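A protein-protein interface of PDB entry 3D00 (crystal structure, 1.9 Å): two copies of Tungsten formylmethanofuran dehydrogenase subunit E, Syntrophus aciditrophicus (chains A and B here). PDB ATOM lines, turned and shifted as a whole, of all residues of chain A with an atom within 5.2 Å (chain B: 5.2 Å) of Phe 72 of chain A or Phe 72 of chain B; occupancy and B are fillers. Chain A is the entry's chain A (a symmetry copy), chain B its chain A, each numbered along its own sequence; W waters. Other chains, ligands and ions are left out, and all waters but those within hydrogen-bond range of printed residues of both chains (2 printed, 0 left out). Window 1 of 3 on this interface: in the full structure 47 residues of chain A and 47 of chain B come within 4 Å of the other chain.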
ATOM      1  N   ARG A  57      15.070 -29.009  -6.175  1.00  0.00           N
ATOM      2  CA  ARG A  57      13.717 -29.190  -6.662  1.00  0.00           C
ATOM      3  C   ARG A  57      13.238 -30.650  -6.655  1.00  0.00           C
ATOM      4  O   ARG A  57      12.051 -30.908  -6.699  1.00  0.00           O
ATOM      5  CB  ARG A  57      13.526 -28.505  -8.013  1.00  0.00           C
ATOM      6  CG  ARG A  57      14.269 -29.049  -9.185  1.00  0.00           C
ATOM      7  CD  ARG A  57      13.954 -28.165 -10.406  1.00  0.00           C
ATOM      8  N   PRO A  61      10.825 -30.938  -2.063  1.00  0.00           N
ATOM      9  CA  PRO A  61       9.634 -30.094  -1.887  1.00  0.00           C
ATOM     10  C   PRO A  61       8.331 -30.794  -1.484  1.00  0.00           C
ATOM     11  O   PRO A  61       7.555 -30.211  -0.743  1.00  0.00           O
ATOM     12  CB  PRO A  61       9.482 -29.452  -3.254  1.00  0.00           C
ATOM     13  CG  PRO A  61      10.865 -29.359  -3.786  1.00  0.00           C
ATOM     14  CD  PRO A  61      11.491 -30.647  -3.365  1.00  0.00           C
ATOM     15  N   ASP A  62       8.078 -32.001  -1.992  1.00  0.00           N
ATOM     16  CA  ASP A  62       6.842 -32.721  -1.669  1.00  0.00           C
ATOM     17  C   ASP A  62       6.771 -33.203  -0.248  1.00  0.00           C
ATOM     18  O   ASP A  62       5.687 -33.320   0.288  1.00  0.00           O
ATOM     19  CB  ASP A  62       6.605 -33.860  -2.644  1.00  0.00           C
ATOM     20  CG  ASP A  62       6.213 -33.353  -4.031  1.00  0.00           C
ATOM     21  OD1 ASP A  62       5.991 -32.134  -4.218  1.00  0.00           O
ATOM     22  OD2 ASP A  62       6.094 -34.190  -4.941  1.00  0.00           O
ATOM     23  N   GLN A  65       5.653 -29.964   1.435  1.00  0.00           N
ATOM     24  CA  GLN A  65       4.243 -29.728   1.122  1.00  0.00           C
ATOM     25  C   GLN A  65       3.299 -30.680   1.780  1.00  0.00           C
ATOM     26  O   GLN A  65       2.218 -30.259   2.257  1.00  0.00           O
ATOM     27  CB  GLN A  65       4.037 -29.727  -0.361  1.00  0.00           C
ATOM     28  CG  GLN A  65       4.740 -28.586  -0.979  1.00  0.00           C
ATOM     29  CD  GLN A  65       4.386 -28.403  -2.405  1.00  0.00           C
ATOM     30  OE1 GLN A  65       3.848 -27.369  -2.779  1.00  0.00           O
ATOM     31  NE2 GLN A  65       4.702 -29.398  -3.232  1.00  0.00           N
ATOM     32  N   CYS A  70       3.514 -25.107   4.630  1.00  0.00           N
ATOM     33  CA  CYS A  70       4.218 -24.396   3.597  1.00  0.00           C
ATOM     34  C   CYS A  70       4.029 -25.113   2.279  1.00  0.00           C
ATOM     35  O   CYS A  70       4.415 -26.283   2.126  1.00  0.00           O
ATOM     36  CB  CYS A  70       5.717 -24.292   3.930  1.00  0.00           C
ATOM     37  SG  CYS A  70       6.066 -23.723   5.619  1.00  0.00           S
ATOM     38  N   THR A  71       3.506 -24.394   1.301  1.00  0.00           N
ATOM     39  CA  THR A  71       3.361 -24.925  -0.037  1.00  0.00           C
ATOM     40  C   THR A  71       4.005 -23.994  -1.039  1.00  0.00           C
ATOM     41  O   THR A  71       4.240 -22.826  -0.780  1.00  0.00           O
ATOM     42  CB  THR A  71       1.869 -25.206  -0.427  1.00  0.00           C
ATOM     43  OG1 THR A  71       1.181 -23.996  -0.718  1.00  0.00           O
ATOM     44  CG2 THR A  71       1.153 -25.922   0.677  1.00  0.00           C
ATOM     45  N   PHE A  72       4.271 -24.532  -2.211  1.00  0.00           N
ATOM     46  CA  PHE A  72       4.766 -23.725  -3.277  1.00  0.00           C
ATOM     47  C   PHE A  72       3.780 -22.601  -3.667  1.00  0.00           C
ATOM     48  O   PHE A  72       4.187 -21.454  -3.822  1.00  0.00           O
ATOM     49  CB  PHE A  72       5.093 -24.549  -4.515  1.00  0.00           C
ATOM     50  CG  PHE A  72       6.007 -23.833  -5.420  1.00  0.00           C
ATOM     51  CD1 PHE A  72       7.377 -23.922  -5.237  1.00  0.00           C
ATOM     52  CD2 PHE A  72       5.522 -22.942  -6.350  1.00  0.00           C
ATOM     53  CE1 PHE A  72       8.239 -23.169  -6.011  1.00  0.00           C
ATOM     54  CE2 PHE A  72       6.395 -22.203  -7.126  1.00  0.00           C
ATOM     55  CZ  PHE A  72       7.735 -22.306  -6.938  1.00  0.00           C
ATOM     56  N   GLY A  73       2.498 -22.944  -3.790  1.00  0.00           N
ATOM     57  CA  GLY A  73       1.471 -21.965  -4.118  1.00  0.00           C
ATOM     58  C   GLY A  73       1.124 -20.887  -3.078  1.00  0.00           C
ATOM     59  O   GLY A  73       0.575 -19.868  -3.468  1.00  0.00           O
ATOM     60  N   ASN A  74       1.389 -21.084  -1.777  1.00  0.00           N
ATOM     61  CA  ASN A  74       1.118 -20.021  -0.751  1.00  0.00           C
ATOM     62  C   ASN A  74       2.351 -19.189  -0.425  1.00  0.00           C
ATOM     63  O   ASN A  74       2.318 -18.217   0.354  1.00  0.00           O
ATOM     64  CB  ASN A  74       0.456 -20.569   0.528  1.00  0.00           C
ATOM     65  CG  ASN A  74       1.327 -21.507   1.312  1.00  0.00           C
ATOM     66  OD1 ASN A  74       2.539 -21.562   1.139  1.00  0.00           O
ATOM     67  ND2 ASN A  74       0.703 -22.264   2.188  1.00  0.00           N
ATOM     68  N   GLY A  75       3.438 -19.585  -1.053  1.00  0.00           N
ATOM     69  CA  GLY A  75       4.689 -18.876  -0.990  1.00  0.00           C
ATOM     70  C   GLY A  75       5.465 -19.106   0.274  1.00  0.00           C
ATOM     71  O   GLY A  75       6.518 -18.513   0.439  1.00  0.00           O
ATOM     72  N   LEU A  77       6.721 -21.965   1.112  1.00  0.00           N
ATOM     73  CA  LEU A  77       7.852 -22.744   0.601  1.00  0.00           C
ATOM     74  C   LEU A  77       8.522 -22.043  -0.570  1.00  0.00           C
ATOM     75  O   LEU A  77       7.853 -21.734  -1.590  1.00  0.00           O
ATOM     76  CB  LEU A  77       7.399 -24.103   0.122  1.00  0.00           C
ATOM     77  CG  LEU A  77       8.422 -25.067  -0.504  1.00  0.00           C
ATOM     78  CD1 LEU A  77       9.638 -25.380   0.394  1.00  0.00           C
ATOM     79  CD2 LEU A  77       7.766 -26.352  -0.979  1.00  0.00           C
ATOM     80  N   VAL A  79      11.832 -22.754  -3.165  1.00  0.00           N
ATOM     81  CA  VAL A  79      12.731 -23.732  -3.679  1.00  0.00           C
ATOM     82  C   VAL A  79      13.867 -22.973  -4.379  1.00  0.00           C
ATOM     83  O   VAL A  79      13.625 -22.143  -5.265  1.00  0.00           O
ATOM     84  CB  VAL A  79      12.012 -24.669  -4.643  1.00  0.00           C
ATOM     85  CG1 VAL A  79      13.003 -25.588  -5.297  1.00  0.00           C
ATOM     86  CG2 VAL A  79      10.891 -25.475  -3.850  1.00  0.00           C
ATOM     87  N   ARG B  57       3.748 -18.074  -9.789  1.00  0.00           N
ATOM     88  CA  ARG B  57       3.963 -18.832  -8.572  1.00  0.00           C
ATOM     89  C   ARG B  57       2.828 -18.699  -7.543  1.00  0.00           C
ATOM     90  O   ARG B  57       2.703 -19.522  -6.657  1.00  0.00           O
ATOM     91  CB  ARG B  57       5.340 -18.539  -7.982  1.00  0.00           C
ATOM     92  CG  ARG B  57       5.600 -17.170  -7.453  1.00  0.00           C
ATOM     93  CD  ARG B  57       7.060 -17.112  -6.967  1.00  0.00           C
ATOM     94  N   PRO B  61      -0.115 -22.822  -8.698  1.00  0.00           N
ATOM     95  CA  PRO B  61       0.493 -24.146  -8.500  1.00  0.00           C
ATOM     96  C   PRO B  61      -0.251 -25.131  -7.590  1.00  0.00           C
ATOM     97  O   PRO B  61      -0.212 -26.322  -7.857  1.00  0.00           O
ATOM     98  CB  PRO B  61       1.845 -23.800  -7.903  1.00  0.00           C
ATOM     99  CG  PRO B  61       2.186 -22.474  -8.477  1.00  0.00           C
ATOM    100  CD  PRO B  61       0.885 -21.741  -8.465  1.00  0.00           C
ATOM    101  N   ASP B  62      -0.879 -24.649  -6.516  1.00  0.00           N
ATOM    102  CA  ASP B  62      -1.591 -25.534  -5.589  1.00  0.00           C
ATOM    103  C   ASP B  62      -2.841 -26.139  -6.162  1.00  0.00           C
ATOM    104  O   ASP B  62      -3.215 -27.223  -5.763  1.00  0.00           O
ATOM    105  CB  ASP B  62      -1.879 -24.828  -4.276  1.00  0.00           C
ATOM    106  CG  ASP B  62      -0.612 -24.613  -3.452  1.00  0.00           C
ATOM    107  OD1 ASP B  62       0.474 -25.121  -3.819  1.00  0.00           O
ATOM    108  OD2 ASP B  62      -0.707 -23.953  -2.404  1.00  0.00           O
ATOM    109  N   GLN B  65      -1.274 -29.008  -8.133  1.00  0.00           N
ATOM    110  CA  GLN B  65      -0.835 -30.044  -7.197  1.00  0.00           C
ATOM    111  C   GLN B  65      -1.949 -30.786  -6.535  1.00  0.00           C
ATOM    112  O   GLN B  65      -1.863 -32.028  -6.373  1.00  0.00           O
ATOM    113  CB  GLN B  65       0.085 -29.457  -6.172  1.00  0.00           C
ATOM    114  CG  GLN B  65       1.334 -28.991  -6.807  1.00  0.00           C
ATOM    115  CD  GLN B  65       2.369 -28.613  -5.818  1.00  0.00           C
ATOM    116  OE1 GLN B  65       3.437 -29.211  -5.784  1.00  0.00           O
ATOM    117  NE2 GLN B  65       2.080 -27.596  -5.008  1.00  0.00           N
ATOM    118  N   CYS B  70       0.683 -34.015 -11.212  1.00  0.00           N
ATOM    119  CA  CYS B  70       1.847 -33.188 -11.378  1.00  0.00           C
ATOM    120  C   CYS B  70       2.100 -32.418 -10.101  1.00  0.00           C
ATOM    121  O   CYS B  70       1.256 -31.626  -9.653  1.00  0.00           O
ATOM    122  CB  CYS B  70       1.661 -32.211 -12.553  1.00  0.00           C
ATOM    123  SG  CYS B  70       1.057 -32.990 -14.078  1.00  0.00           S
ATOM    124  N   THR B  71       3.290 -32.588  -9.550  1.00  0.00           N
ATOM    125  CA  THR B  71       3.700 -31.840  -8.382  1.00  0.00           C
ATOM    126  C   THR B  71       5.020 -31.153  -8.641  1.00  0.00           C
ATOM    127  O   THR B  71       5.772 -31.509  -9.534  1.00  0.00           O
ATOM    128  CB  THR B  71       3.781 -32.720  -7.088  1.00  0.00           C
ATOM    129  OG1 THR B  71       4.943 -33.539  -7.100  1.00  0.00           O
ATOM    130  CG2 THR B  71       2.570 -33.591  -6.955  1.00  0.00           C
ATOM    131  N   PHE B  72       5.305 -30.162  -7.823  1.00  0.00           N
ATOM    132  CA  PHE B  72       6.575 -29.516  -7.888  1.00  0.00           C
ATOM    133  C   PHE B  72       7.742 -30.490  -7.616  1.00  0.00           C
ATOM    134  O   PHE B  72       8.724 -30.494  -8.351  1.00  0.00           O
ATOM    135  CB  PHE B  72       6.672 -28.343  -6.922  1.00  0.00           C
ATOM    136  CG  PHE B  72       7.752 -27.416  -7.298  1.00  0.00           C
ATOM    137  CD1 PHE B  72       7.511 -26.398  -8.205  1.00  0.00           C
ATOM    138  CD2 PHE B  72       9.047 -27.641  -6.887  1.00  0.00           C
ATOM    139  CE1 PHE B  72       8.542 -25.592  -8.646  1.00  0.00           C
ATOM    140  CE2 PHE B  72      10.067 -26.820  -7.326  1.00  0.00           C
ATOM    141  CZ  PHE B  72       9.814 -25.823  -8.212  1.00  0.00           C
ATOM    142  N   GLY B  73       7.603 -31.318  -6.580  1.00  0.00           N
ATOM    143  CA  GLY B  73       8.619 -32.305  -6.245  1.00  0.00           C
ATOM    144  C   GLY B  73       8.845 -33.483  -7.207  1.00  0.00           C
ATOM    145  O   GLY B  73       9.911 -34.076  -7.150  1.00  0.00           O
ATOM    146  N   ASN B  74       7.879 -33.862  -8.059  1.00  0.00           N
ATOM    147  CA  ASN B  74       8.098 -34.968  -9.051  1.00  0.00           C
ATOM    148  C   ASN B  74       8.501 -34.453 -10.427  1.00  0.00           C
ATOM    149  O   ASN B  74       8.790 -35.215 -11.371  1.00  0.00           O
ATOM    150  CB  ASN B  74       6.910 -35.944  -9.143  1.00  0.00           C
ATOM    151  CG  ASN B  74       5.652 -35.325  -9.679  1.00  0.00           C
ATOM    152  OD1 ASN B  74       5.662 -34.263 -10.291  1.00  0.00           O
ATOM    153  ND2 ASN B  74       4.544 -35.994  -9.443  1.00  0.00           N
ATOM    154  N   GLY B  75       8.528 -33.140 -10.514  1.00  0.00           N
ATOM    155  CA  GLY B  75       8.994 -32.436 -11.679  1.00  0.00           C
ATOM    156  C   GLY B  75       8.004 -32.383 -12.805  1.00  0.00           C
ATOM    157  O   GLY B  75       8.324 -31.845 -13.852  1.00  0.00           O
ATOM    158  N   LEU B  77       5.182 -30.812 -12.639  1.00  0.00           N
ATOM    159  CA  LEU B  77       4.834 -29.389 -12.630  1.00  0.00           C
ATOM    160  C   LEU B  77       6.076 -28.515 -12.686  1.00  0.00           C
ATOM    161  O   LEU B  77       6.975 -28.636 -11.814  1.00  0.00           O
ATOM    162  CB  LEU B  77       4.076 -29.027 -11.374  1.00  0.00           C
ATOM    163  CG  LEU B  77       3.657 -27.566 -11.135  1.00  0.00           C
ATOM    164  CD1 LEU B  77       2.806 -26.951 -12.268  1.00  0.00           C
ATOM    165  CD2 LEU B  77       2.964 -27.391  -9.795  1.00  0.00           C
ATOM    166  N   VAL B  79       6.967 -24.345 -12.787  1.00  0.00           N
ATOM    167  CA  VAL B  79       6.474 -23.033 -12.534  1.00  0.00           C
ATOM    168  C   VAL B  79       7.453 -22.051 -13.191  1.00  0.00           C
ATOM    169  O   VAL B  79       8.662 -22.084 -12.924  1.00  0.00           O
ATOM    170  CB  VAL B  79       6.359 -22.783 -11.034  1.00  0.00           C
ATOM    171  CG1 VAL B  79       5.994 -21.349 -10.782  1.00  0.00           C
ATOM    172  CG2 VAL B  79       5.284 -23.785 -10.418  1.00  0.00           C
HETATM  173  O   HOH W   1      11.437 -31.626  -9.332  1.00  0.00           O
HETATM  174  O   HOH W   2       3.780 -18.423  -4.321  1.00  0.00           O
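The side-chain carboxylate of Asp 62 of chain B lies within hydrogen-bond range of the backbone NH of Gly 73 of chain A, 3.0 Å away.
The side-chain hydroxyl of Thr 71 of chain A lies within hydrogen-bond range of the side-chain carboxylate of Asp 62 of chain B, 2.5 Å away.
The backbone NH (N) of Gly 73 of chain B lies within hydrogen-bond range of the side-chain carboxylate (OD1) of Asp 62 of chain A.
The side-chain amide oxygen of Gln 65 of chain A sits at hydrogen-bond distance from the side-chain amide nitrogen of Gln 65 of chain B, 2.9 Å away.
The side-chain hydroxyl (OG1) of Thr 71 of chain B sits at hydrogen-bond distance from the side-chain carboxylate (OD2) of Asp 62 of chain A, 2.5 Å away.
Among the printed residues, merely in contact across the chains: Phe 72 of chain A with Phe 72 of chain B, Asp 62 of chain A with Asn 74 of chain B, Asn 74 of chain A with Asp 62 of chain B, Gly 73 of chain A with Arg 57 of chain B, Arg 57 of chain A with Gly 73 of chain B, Arg 57 of chain A with Phe 72 of chain B, Phe 72 of chain A with Arg 57 of chain B, Val 79 of chain A with Phe 72 of chain B, Phe 72 of chain A with Val 79 of chain B, Phe 72 of chain A with Pro 61 of chain B and Pro 61 of chain A with Phe 72 of chain B.
The backbone carbonyl oxygen (O) of Thr 71 of chain B sits close to the side-chain amide oxygen (OD1) of Asn 74 of chain B, 2.9 Å away.
The side-chain amide oxygen (OE1) of Gln 65 of chain B sits at hydrogen-bond distance from the backbone NH (N) of Phe 72 of chain B, 2.9 Å away.
OD1 of Asp 62 of chain A lies within hydrogen-bond range of NE2 of Gln 65 of chain A (3.2 Å).
N of Phe 72 of chain A sits at hydrogen-bond distance from OE1 of Gln 65 of chain A.
The side-chain amide oxygen (OD1) of Asn 74 of chain A sits close to the backbone carbonyl oxygen (O) of Thr 71 of chain A.
The backbone carbonyl oxygen (O) of Thr 71 of chain A sits at hydrogen-bond distance from the backbone NH (N) of Leu 77 of chain A (3.2 Å).
Of the 12 printed residues of chain A, 9 touch a printed residue of chain B.
Printed residues of chain A that touch a printed residue of chain B: Arg 57, Pro 61, Asp 62, Gln 65, Thr 71, Phe 72, Gly 73, Asn 74 and Val 79.
Hydrophobic or aromatic side chains of chain B within 4 Å of the printed part of chain A: Pro 61, Phe 72 and Val 79.
Among the printed residues, 16 pairs touch across the chains.
Cys 70 of chain A touches none of the printed residues of chain B.
Printed residues of chain B within 4 Å of Phe 72 of chain A: Arg 57, Pro 61, Phe 72 and Val 79.
Of the printed residues of chain B, Gly 73 of chain A touches Arg 57 (3.7 Å) and Asp 62 (3.0 Å).
Of the printed residues of chain A, Phe 72 of chain B touches Arg 57, Pro 61, Phe 72 and Val 79.
Of the printed residues of chain A, Gly 73 of chain B touches Arg 57 and Asp 62.
Of the printed residues of chain A, Val 79 of chain B touches Phe 72.
The nearest printed residue of chain A that does not touch Phe 72 of chain B is Asp 62 of chain A (4.2 Å).
The nearest printed residue of chain A that does not touch Asn 74 of chain B is Arg 57 of chain A (5.3 Å).
Water W2 lies within hydrogen-bond range of O of Arg 57 of chain B, O of Phe 72 of chain A and N of Gly 75 of chain A.
Water W1 lies within hydrogen-bond range of O of Arg 57 of chain A, O of Phe 72 of chain B and N of Gly 75 of chain B.
Pro 61 of chain A touches Phe 72 of chain B, and with the chains exchanged Phe 72 of chain A touches Pro 61 of chain B.
Asp 62 of chain A touches Thr 71 of chain B, and with the chains exchanged Thr 71 of chain A touches Asp 62 of chain B.
Asp 62 of chain A touches Asn 74 of chain B, and with the chains exchanged Asn 74 of chain A touches Asp 62 of chain B.
Gln 65 of chain A touches its own counterpart, Gln 65 of chain B.
Of the 16 pairs that touch across the chains among the printed residues, 16 have their exchanged pair printed and touching as well.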
